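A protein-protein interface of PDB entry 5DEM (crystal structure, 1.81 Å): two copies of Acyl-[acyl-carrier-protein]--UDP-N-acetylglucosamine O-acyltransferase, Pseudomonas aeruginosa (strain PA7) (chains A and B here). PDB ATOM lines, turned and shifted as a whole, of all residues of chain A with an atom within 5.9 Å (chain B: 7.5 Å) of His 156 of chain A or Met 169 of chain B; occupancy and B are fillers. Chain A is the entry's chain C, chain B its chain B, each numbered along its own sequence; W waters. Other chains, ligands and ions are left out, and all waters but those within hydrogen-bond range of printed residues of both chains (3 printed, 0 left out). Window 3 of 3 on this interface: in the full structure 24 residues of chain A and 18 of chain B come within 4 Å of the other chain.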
ATOM      1  N   ALA A 136     -11.215  18.602  27.797  1.00  0.00           N
ATOM      2  CA  ALA A 136     -12.612  18.486  28.118  1.00  0.00           C
ATOM      3  C   ALA A 136     -13.234  17.320  27.383  1.00  0.00           C
ATOM      4  O   ALA A 136     -13.282  17.298  26.145  1.00  0.00           O
ATOM      5  CB  ALA A 136     -13.352  19.790  27.772  1.00  0.00           C
ATOM      6  N   ALA A 138     -16.689  15.804  26.648  1.00  0.00           N
ATOM      7  CA  ALA A 138     -18.048  16.334  26.719  1.00  0.00           C
ATOM      8  C   ALA A 138     -19.074  15.400  27.363  1.00  0.00           C
ATOM      9  O   ALA A 138     -19.977  15.872  28.040  1.00  0.00           O
ATOM     10  CB  ALA A 138     -18.539  16.788  25.352  1.00  0.00           C
ATOM     11  N   GLY A 139     -18.915  14.092  27.191  1.00  0.00           N
ATOM     12  CA  GLY A 139     -19.880  13.157  27.692  1.00  0.00           C
ATOM     13  C   GLY A 139     -19.812  11.868  26.906  1.00  0.00           C
ATOM     14  O   GLY A 139     -19.634  11.898  25.695  1.00  0.00           O
ATOM     15  N   VAL A 141     -17.525   9.804  26.604  1.00  0.00           N
ATOM     16  CA  VAL A 141     -16.230   9.621  25.932  1.00  0.00           C
ATOM     17  C   VAL A 141     -15.460   8.459  26.542  1.00  0.00           C
ATOM     18  O   VAL A 141     -15.385   8.337  27.765  1.00  0.00           O
ATOM     19  CB  VAL A 141     -15.387  10.911  26.013  1.00  0.00           C
ATOM     20  CG1 VAL A 141     -13.973  10.689  25.505  1.00  0.00           C
ATOM     21  CG2 VAL A 141     -16.074  12.023  25.247  1.00  0.00           C
ATOM     22  N   LEU A 154     -10.342  19.185  23.124  1.00  0.00           N
ATOM     23  CA  LEU A 154     -11.769  19.105  23.299  1.00  0.00           C
ATOM     24  C   LEU A 154     -12.253  17.846  22.603  1.00  0.00           C
ATOM     25  O   LEU A 154     -11.938  17.619  21.416  1.00  0.00           O
ATOM     26  CB  LEU A 154     -12.450  20.314  22.662  1.00  0.00           C
ATOM     27  CG  LEU A 154     -11.819  21.659  22.966  1.00  0.00           C
ATOM     28  CD1 LEU A 154     -12.564  22.769  22.254  1.00  0.00           C
ATOM     29  CD2 LEU A 154     -11.808  21.891  24.473  1.00  0.00           C
ATOM     30  N   VAL A 155     -13.055  17.051  23.298  1.00  0.00           N
ATOM     31  CA  VAL A 155     -13.547  15.781  22.717  1.00  0.00           C
ATOM     32  C   VAL A 155     -15.062  15.754  22.729  1.00  0.00           C
ATOM     33  O   VAL A 155     -15.702  15.892  23.786  1.00  0.00           O
ATOM     34  CB  VAL A 155     -12.991  14.548  23.476  1.00  0.00           C
ATOM     35  CG1 VAL A 155     -13.435  13.260  22.790  1.00  0.00           C
ATOM     36  CG2 VAL A 155     -11.471  14.607  23.572  1.00  0.00           C
ATOM     37  N   HIS A 156     -15.646  15.704  21.533  1.00  0.00           N
ATOM     38  CA  HIS A 156     -17.115  15.618  21.347  1.00  0.00           C
ATOM     39  C   HIS A 156     -17.755  14.370  21.971  1.00  0.00           C
ATOM     40  O   HIS A 156     -17.110  13.334  22.150  1.00  0.00           O
ATOM     41  CB  HIS A 156     -17.487  15.659  19.857  1.00  0.00           C
ATOM     42  CG  HIS A 156     -17.485  17.025  19.263  1.00  0.00           C
ATOM     43  ND1 HIS A 156     -16.332  17.630  18.790  1.00  0.00           N
ATOM     44  CD2 HIS A 156     -18.495  17.894  19.016  1.00  0.00           C
ATOM     45  CE1 HIS A 156     -16.645  18.783  18.221  1.00  0.00           C
ATOM     46  NE2 HIS A 156     -17.948  18.973  18.359  1.00  0.00           N
ATOM     47  N   GLN A 157     -19.019  14.506  22.363  1.00  0.00           N
ATOM     48  CA  GLN A 157     -19.763  13.395  22.928  1.00  0.00           C
ATOM     49  C   GLN A 157     -19.646  12.133  22.103  1.00  0.00           C
ATOM     50  O   GLN A 157     -19.669  12.195  20.883  1.00  0.00           O
ATOM     51  CB  GLN A 157     -21.246  13.750  23.029  1.00  0.00           C
ATOM     52  CG  GLN A 157     -21.605  14.580  24.227  1.00  0.00           C
ATOM     53  CD  GLN A 157     -23.092  14.473  24.539  1.00  0.00           C
ATOM     54  OE1 GLN A 157     -23.914  14.332  23.622  1.00  0.00           O
ATOM     55  NE2 GLN A 157     -23.414  14.326  25.822  1.00  0.00           N
ATOM     56  N   TYR A 158     -19.496  11.014  22.792  1.00  0.00           N
ATOM     57  CA  TYR A 158     -19.515   9.662  22.212  1.00  0.00           C
ATOM     58  C   TYR A 158     -18.230   9.246  21.516  1.00  0.00           C
ATOM     59  O   TYR A 158     -18.095   8.089  21.152  1.00  0.00           O
ATOM     60  CB  TYR A 158     -20.697   9.429  21.256  1.00  0.00           C
ATOM     61  CG  TYR A 158     -22.045   9.579  21.914  1.00  0.00           C
ATOM     62  CD1 TYR A 158     -22.456   8.691  22.891  1.00  0.00           C
ATOM     63  CD2 TYR A 158     -22.839  10.681  21.652  1.00  0.00           C
ATOM     64  CE1 TYR A 158     -23.694   8.814  23.490  1.00  0.00           C
ATOM     65  CE2 TYR A 158     -24.048  10.864  22.316  1.00  0.00           C
ATOM     66  CZ  TYR A 158     -24.458   9.927  23.243  1.00  0.00           C
ATOM     67  OH  TYR A 158     -25.655  10.089  23.903  1.00  0.00           O
ATOM     68  N   CYS A 159     -17.243  10.133  21.434  1.00  0.00           N
ATOM     69  CA  CYS A 159     -16.004   9.763  20.772  1.00  0.00           C
ATOM     70  C   CYS A 159     -15.202   8.766  21.589  1.00  0.00           C
ATOM     71  O   CYS A 159     -15.207   8.810  22.835  1.00  0.00           O
ATOM     72  CB  CYS A 159     -15.172  11.005  20.469  1.00  0.00           C
ATOM     73  SG  CYS A 159     -15.900  12.020  19.162  1.00  0.00           S
ATOM     74  N   ALA A 172      -9.431  19.653  18.476  1.00  0.00           N
ATOM     75  CA  ALA A 172     -10.863  19.490  18.660  1.00  0.00           C
ATOM     76  C   ALA A 172     -11.253  18.202  17.928  1.00  0.00           C
ATOM     77  O   ALA A 172     -11.342  18.174  16.698  1.00  0.00           O
ATOM     78  CB  ALA A 172     -11.631  20.671  18.090  1.00  0.00           C
ATOM     79  N   ILE A 173     -11.605  17.199  18.712  1.00  0.00           N
ATOM     80  CA  ILE A 173     -11.799  15.860  18.226  1.00  0.00           C
ATOM     81  C   ILE A 173     -13.277  15.562  18.125  1.00  0.00           C
ATOM     82  O   ILE A 173     -14.005  15.613  19.122  1.00  0.00           O
ATOM     83  CB  ILE A 173     -11.103  14.856  19.166  1.00  0.00           C
ATOM     84  CG1 ILE A 173      -9.597  15.113  19.149  1.00  0.00           C
ATOM     85  CG2 ILE A 173     -11.456  13.422  18.795  1.00  0.00           C
ATOM     86  CD1 ILE A 173      -8.808  14.354  20.189  1.00  0.00           C
ATOM     87  N   GLY A 174     -13.727  15.256  16.917  1.00  0.00           N
ATOM     88  CA  GLY A 174     -15.149  15.050  16.646  1.00  0.00           C
ATOM     89  C   GLY A 174     -15.465  13.635  16.177  1.00  0.00           C
ATOM     90  O   GLY A 174     -16.626  13.270  16.048  1.00  0.00           O
ATOM     91  N   LYS A 175     -14.429  12.873  15.854  1.00  0.00           N
ATOM     92  CA  LYS A 175     -14.558  11.476  15.426  1.00  0.00           C
ATOM     93  C   LYS A 175     -13.617  10.632  16.251  1.00  0.00           C
ATOM     94  O   LYS A 175     -12.671  11.166  16.836  1.00  0.00           O
ATOM     95  CB  LYS A 175     -14.178  11.380  13.952  1.00  0.00           C
ATOM     96  CG  LYS A 175     -15.007  12.301  13.073  1.00  0.00           C
ATOM     97  CD  LYS A 175     -14.520  12.302  11.634  1.00  0.00           C
ATOM     98  CE  LYS A 175     -15.235  11.235  10.830  1.00  0.00           C
ATOM     99  NZ  LYS A 175     -16.653  11.637  10.613  1.00  0.00           N
ATOM    100  N   ASN A 186      -7.957  21.922  14.817  1.00  0.00           N
ATOM    101  CA  ASN A 186      -9.399  22.068  14.936  1.00  0.00           C
ATOM    102  C   ASN A 186      -9.911  22.371  13.519  1.00  0.00           C
ATOM    103  O   ASN A 186      -9.694  23.479  13.047  1.00  0.00           O
ATOM    104  CB  ASN A 186      -9.728  23.219  15.892  1.00  0.00           C
ATOM    105  CG  ASN A 186     -11.212  23.510  15.970  1.00  0.00           C
ATOM    106  OD1 ASN A 186     -12.018  22.831  15.364  1.00  0.00           O
ATOM    107  ND2 ASN A 186     -11.576  24.533  16.723  1.00  0.00           N
ATOM    108  N   ARG A 254     -18.888   5.518  13.923  1.00  0.00           N
ATOM    109  CA  ARG A 254     -19.205   6.866  13.448  1.00  0.00           C
ATOM    110  C   ARG A 254     -18.026   7.523  12.712  1.00  0.00           C
ATOM    111  O   ARG A 254     -17.955   8.747  12.598  1.00  0.00           O
ATOM    112  CB  ARG A 254     -19.687   7.727  14.624  1.00  0.00           C
ATOM    113  CG  ARG A 254     -21.005   7.239  15.249  1.00  0.00           C
ATOM    114  CD  ARG A 254     -21.381   8.046  16.498  1.00  0.00           C
ATOM    115  NE  ARG A 254     -20.142   8.528  17.083  1.00  0.00           N
ATOM    116  CZ  ARG A 254     -19.821   9.796  17.349  1.00  0.00           C
ATOM    117  NH1 ARG A 254     -20.734  10.770  17.341  1.00  0.00           N
ATOM    118  NH2 ARG A 254     -18.600  10.055  17.796  1.00  0.00           N
ATOM    119  N   VAL B 132     -21.989  26.696  27.538  1.00  0.00           N
ATOM    120  CA  VAL B 132     -21.304  25.466  27.923  1.00  0.00           C
ATOM    121  C   VAL B 132     -19.898  25.742  28.474  1.00  0.00           C
ATOM    122  O   VAL B 132     -19.432  26.892  28.422  1.00  0.00           O
ATOM    123  CB  VAL B 132     -21.323  24.453  26.737  1.00  0.00           C
ATOM    124  CG1 VAL B 132     -20.622  23.151  27.080  1.00  0.00           C
ATOM    125  CG2 VAL B 132     -22.763  24.167  26.328  1.00  0.00           C
ATOM    126  N   ASN B 133     -19.335  24.773  29.189  1.00  0.00           N
ATOM    127  CA  ASN B 133     -18.039  24.934  29.910  1.00  0.00           C
ATOM    128  C   ASN B 133     -17.043  25.840  29.203  1.00  0.00           C
ATOM    129  O   ASN B 133     -16.759  25.612  28.024  1.00  0.00           O
ATOM    130  CB  ASN B 133     -17.326  23.583  30.034  1.00  0.00           C
ATOM    131  CG  ASN B 133     -18.079  22.581  30.880  1.00  0.00           C
ATOM    132  OD1 ASN B 133     -19.288  22.406  30.724  1.00  0.00           O
ATOM    133  ND2 ASN B 133     -17.365  21.918  31.790  1.00  0.00           N
ATOM    134  N   LEU B 149     -24.087  28.333  23.278  1.00  0.00           N
ATOM    135  CA  LEU B 149     -22.666  28.428  22.957  1.00  0.00           C
ATOM    136  C   LEU B 149     -21.983  27.205  23.499  1.00  0.00           C
ATOM    137  O   LEU B 149     -21.975  26.980  24.725  1.00  0.00           O
ATOM    138  CB  LEU B 149     -22.049  29.686  23.546  1.00  0.00           C
ATOM    139  CG  LEU B 149     -22.635  31.000  23.035  1.00  0.00           C
ATOM    140  CD1 LEU B 149     -21.894  32.177  23.655  1.00  0.00           C
ATOM    141  CD2 LEU B 149     -22.559  31.094  21.524  1.00  0.00           C
ATOM    142  N   SER B 150     -21.536  26.338  22.602  1.00  0.00           N
ATOM    143  CA  SER B 150     -20.901  25.087  23.034  1.00  0.00           C
ATOM    144  C   SER B 150     -19.565  25.310  23.748  1.00  0.00           C
ATOM    145  O   SER B 150     -19.028  26.416  23.812  1.00  0.00           O
ATOM    146  CB  SER B 150     -20.741  24.102  21.871  1.00  0.00           C
ATOM    147  OG  SER B 150     -21.998  23.724  21.326  1.00  0.00           O
ATOM    148  N   GLY B 151     -19.025  24.228  24.306  1.00  0.00           N
ATOM    149  CA  GLY B 151     -17.820  24.322  25.131  1.00  0.00           C
ATOM    150  C   GLY B 151     -16.684  25.110  24.496  1.00  0.00           C
ATOM    151  O   GLY B 151     -16.402  24.946  23.299  1.00  0.00           O
ATOM    152  N   TYR B 152     -16.018  25.945  25.291  1.00  0.00           N
ATOM    153  CA  TYR B 152     -14.823  26.666  24.854  1.00  0.00           C
ATOM    154  C   TYR B 152     -15.115  27.522  23.617  1.00  0.00           C
ATOM    155  O   TYR B 152     -14.191  27.841  22.871  1.00  0.00           O
ATOM    156  CB  TYR B 152     -13.678  25.691  24.566  1.00  0.00           C
ATOM    157  CG  TYR B 152     -13.098  25.068  25.841  1.00  0.00           C
ATOM    158  CD1 TYR B 152     -13.772  24.070  26.538  1.00  0.00           C
ATOM    159  CD2 TYR B 152     -11.902  25.523  26.345  1.00  0.00           C
ATOM    160  CE1 TYR B 152     -13.218  23.515  27.698  1.00  0.00           C
ATOM    161  CE2 TYR B 152     -11.326  24.944  27.478  1.00  0.00           C
ATOM    162  CZ  TYR B 152     -12.012  23.988  28.162  1.00  0.00           C
ATOM    163  OH  TYR B 152     -11.473  23.552  29.371  1.00  0.00           O
ATOM    164  N   THR B 153     -16.317  28.072  23.568  1.00  0.00           N
ATOM    165  CA  THR B 153     -16.605  29.137  22.632  1.00  0.00           C
ATOM    166  C   THR B 153     -16.032  30.455  23.156  1.00  0.00           C
ATOM    167  O   THR B 153     -16.260  30.838  24.312  1.00  0.00           O
ATOM    168  CB  THR B 153     -18.116  29.268  22.374  1.00  0.00           C
ATOM    169  OG1 THR B 153     -18.606  28.089  21.711  1.00  0.00           O
ATOM    170  CG2 THR B 153     -18.393  30.467  21.540  1.00  0.00           C
ATOM    171  N   PHE B 166     -26.329  29.097  17.490  1.00  0.00           N
ATOM    172  CA  PHE B 166     -25.586  27.987  18.028  1.00  0.00           C
ATOM    173  C   PHE B 166     -24.145  28.006  17.583  1.00  0.00           C
ATOM    174  O   PHE B 166     -23.855  28.285  16.409  1.00  0.00           O
ATOM    175  CB  PHE B 166     -26.198  26.660  17.545  1.00  0.00           C
ATOM    176  CG  PHE B 166     -25.450  25.438  18.007  1.00  0.00           C
ATOM    177  CD1 PHE B 166     -25.742  24.823  19.220  1.00  0.00           C
ATOM    178  CD2 PHE B 166     -24.458  24.897  17.233  1.00  0.00           C
ATOM    179  CE1 PHE B 166     -25.157  23.610  19.566  1.00  0.00           C
ATOM    180  CE2 PHE B 166     -23.845  23.692  17.596  1.00  0.00           C
ATOM    181  CZ  PHE B 166     -24.147  23.091  18.788  1.00  0.00           C
ATOM    182  N   SER B 167     -23.235  27.857  18.539  1.00  0.00           N
ATOM    183  CA  SER B 167     -21.811  27.726  18.203  1.00  0.00           C
ATOM    184  C   SER B 167     -21.377  26.343  18.555  1.00  0.00           C
ATOM    185  O   SER B 167     -21.718  25.807  19.634  1.00  0.00           O
ATOM    186  CB  SER B 167     -20.958  28.774  18.909  1.00  0.00           C
ATOM    187  OG  SER B 167     -20.855  28.474  20.305  1.00  0.00           O
ATOM    188  N   GLY B 168     -20.589  25.763  17.678  1.00  0.00           N
ATOM    189  CA  GLY B 168     -19.905  24.503  17.954  1.00  0.00           C
ATOM    190  C   GLY B 168     -18.767  24.621  18.951  1.00  0.00           C
ATOM    191  O   GLY B 168     -18.236  25.701  19.203  1.00  0.00           O
ATOM    192  N   MET B 169     -18.357  23.480  19.482  1.00  0.00           N
ATOM    193  CA  MET B 169     -17.346  23.462  20.499  1.00  0.00           C
ATOM    194  C   MET B 169     -16.042  24.005  19.949  1.00  0.00           C
ATOM    195  O   MET B 169     -15.694  23.754  18.789  1.00  0.00           O
ATOM    196  CB  MET B 169     -17.154  22.005  20.989  1.00  0.00           C
ATOM    197  CG  MET B 169     -16.334  21.861  22.245  1.00  0.00           C
ATOM    198  SD  MET B 169     -16.407  20.197  22.893  1.00  0.00           S
ATOM    199  CE  MET B 169     -16.105  19.306  21.417  1.00  0.00           C
ATOM    200  N   GLY B 170     -15.425  24.921  20.688  1.00  0.00           N
ATOM    201  CA  GLY B 170     -14.161  25.485  20.300  1.00  0.00           C
ATOM    202  C   GLY B 170     -14.246  26.609  19.277  1.00  0.00           C
ATOM    203  O   GLY B 170     -13.232  27.014  18.759  1.00  0.00           O
ATOM    204  N   SER B 171     -15.421  27.180  19.074  1.00  0.00           N
ATOM    205  CA  SER B 171     -15.578  28.257  18.102  1.00  0.00           C
ATOM    206  C   SER B 171     -14.908  29.518  18.599  1.00  0.00           C
ATOM    207  O   SER B 171     -14.988  29.845  19.774  1.00  0.00           O
ATOM    208  CB  SER B 171     -17.051  28.537  17.853  1.00  0.00           C
ATOM    209  OG  SER B 171     -17.689  27.445  17.209  1.00  0.00           O
ATOM    210  N   ALA B 172     -14.314  30.286  17.701  1.00  0.00           N
ATOM    211  CA  ALA B 172     -13.711  31.560  18.080  1.00  0.00           C
ATOM    212  C   ALA B 172     -14.372  32.640  17.277  1.00  0.00           C
ATOM    213  O   ALA B 172     -14.130  32.745  16.060  1.00  0.00           O
ATOM    214  CB  ALA B 172     -12.196  31.573  17.835  1.00  0.00           C
ATOM    215  N   VAL B 183     -22.569  28.390  13.874  1.00  0.00           N
ATOM    216  CA  VAL B 183     -21.165  28.676  13.539  1.00  0.00           C
ATOM    217  C   VAL B 183     -20.248  27.653  14.162  1.00  0.00           C
ATOM    218  O   VAL B 183     -20.553  27.110  15.218  1.00  0.00           O
ATOM    219  CB  VAL B 183     -20.738  30.103  13.929  1.00  0.00           C
ATOM    220  CG1 VAL B 183     -21.644  31.151  13.317  1.00  0.00           C
ATOM    221  CG2 VAL B 183     -20.697  30.264  15.461  1.00  0.00           C
ATOM    222  N   PHE B 184     -19.088  27.419  13.527  1.00  0.00           N
ATOM    223  CA  PHE B 184     -18.115  26.451  13.989  1.00  0.00           C
ATOM    224  C   PHE B 184     -16.740  26.937  13.627  1.00  0.00           C
ATOM    225  O   PHE B 184     -16.533  27.570  12.574  1.00  0.00           O
ATOM    226  CB  PHE B 184     -18.302  25.074  13.329  1.00  0.00           C
ATOM    227  CG  PHE B 184     -19.324  24.182  13.981  1.00  0.00           C
ATOM    228  CD1 PHE B 184     -20.635  24.187  13.581  1.00  0.00           C
ATOM    229  CD2 PHE B 184     -18.892  23.132  14.818  1.00  0.00           C
ATOM    230  CE1 PHE B 184     -21.543  23.279  14.122  1.00  0.00           C
ATOM    231  CE2 PHE B 184     -19.794  22.226  15.360  1.00  0.00           C
ATOM    232  CZ  PHE B 184     -21.120  22.307  15.001  1.00  0.00           C
ATOM    233  N   GLY B 185     -15.760  26.554  14.434  1.00  0.00           N
ATOM    234  CA  GLY B 185     -14.359  26.698  14.040  1.00  0.00           C
ATOM    235  C   GLY B 185     -13.658  27.936  14.535  1.00  0.00           C
ATOM    236  O   GLY B 185     -14.247  28.821  15.201  1.00  0.00           O
ATOM    237  N   ASN B 186     -12.347  27.957  14.264  1.00  0.00           N
ATOM    238  CA  ASN B 186     -11.510  29.074  14.640  1.00  0.00           C
ATOM    239  C   ASN B 186     -10.672  29.441  13.439  1.00  0.00           C
ATOM    240  O   ASN B 186      -9.754  28.689  13.101  1.00  0.00           O
ATOM    241  CB  ASN B 186     -10.609  28.668  15.811  1.00  0.00           C
ATOM    242  CG  ASN B 186      -9.565  29.704  16.137  1.00  0.00           C
ATOM    243  OD1 ASN B 186      -9.584  30.822  15.630  1.00  0.00           O
ATOM    244  ND2 ASN B 186      -8.724  29.382  17.103  1.00  0.00           N
HETATM  245  O   HOH W   1     -11.536  25.681  12.648  1.00  0.00           O
HETATM  246  O   HOH W   2     -20.263  21.182  19.098  1.00  0.00           O
HETATM  247  O   HOH W   3      -8.417  26.363  14.276  1.00  0.00           O
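Of the 16 printed residues of chain A, 5 touch a printed residue of chain B.
Of the 18 printed residues of chain B, 3 touch a printed residue of chain A.
Hydrophobic or aromatic side chains of chain B within 4 Å of the printed part of chain A: Tyr 152 and Met 169.
Among the printed residues, 7 pairs touch across the chains.
Among the printed residues, no Asp or Glu carboxylate lies within 4 Å of a Lys or Arg side-chain nitrogen of the other chain.
Positions printed for both chains: 172 and 186.
Of the 7 pairs that touch across the chains among the printed residues, none has its exchanged pair printed and touching as well.
Among the printed residues, merely in contact across the chains: His 156 of chain A with Met 169 of chain B (3.1 Å), Leu 154 of chain A with Tyr 152 of chain B (3.6 Å), Asn 186 of chain A with Gly 170 of chain B (3.6 Å), Leu 154 of chain A with Gly 170 of chain B (3.7 Å), Ala 136 of chain A with Tyr 152 of chain B (3.7 Å), Leu 154 of chain A with Met 169 of chain B (3.9 Å) and Val 155 of chain A with Met 169 of chain B (3.9 Å).
The backbone carbonyl oxygen (O) of His 156 of chain A lies close to the side-chain sulfur (SG) of Cys 159 of chain A (3.5 Å).
The backbone NH (N) of His 156 of chain A lies within hydrogen-bond range of the backbone carbonyl oxygen (O) of Ile 173 of chain A.
The backbone carbonyl oxygen (O) of Gly 151 of chain B lies within hydrogen-bond range of the backbone NH (N) of Gly 170 of chain B (2.8 Å).
O of Leu 154 of chain A sits at hydrogen-bond distance from N of Ile 173 of chain A, at 2.8 Å.
O of Asn 133 of chain B is in hydrogen-bond range of N of Tyr 152 of chain B (2.9 Å).
The backbone NH of Val 155 of chain A sits at hydrogen-bond distance from the backbone carbonyl oxygen of Ala 136 of chain A.
Water W1 lies within hydrogen-bond range of the backbone carbonyl oxygen of Asn 186 of chain A (2.9 Å) and the backbone NH of Asn 186 of chain B (2.9 Å).
Water W3 bridges the backbone carbonyl oxygen of Asn 186 of chain B and the backbone carbonyl oxygen of Asn 186 of chain A.
Water W2 bridges the backbone NH of Met 169 of chain B and a ring nitrogen (NE2) of His 156 of chain A.
Printed residues of chain B within 4 Å of Ala 136 of chain A: Tyr 152 (3.7 Å).
Gly 139 of chain A touches none of the printed residues of chain B.
Printed residues of chain B within 4 Å of Val 155 of chain A: Met 169 (3.9 Å).
Of chain B, only Met 169 (3.1 Å) comes within 4 Å of His 156 of chain A.
Of the printed residues of chain B, Asn 186 of chain A touches Gly 170 (3.6 Å).
Of the printed residues of chain A, Met 169 of chain B touches Leu 154 (3.9 Å), Val 155 (3.9 Å) and His 156 (3.1 Å).
The nearest residue of chain B that does not touch His 156 of chain A is Phe 184 of chain B (4.8 Å).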
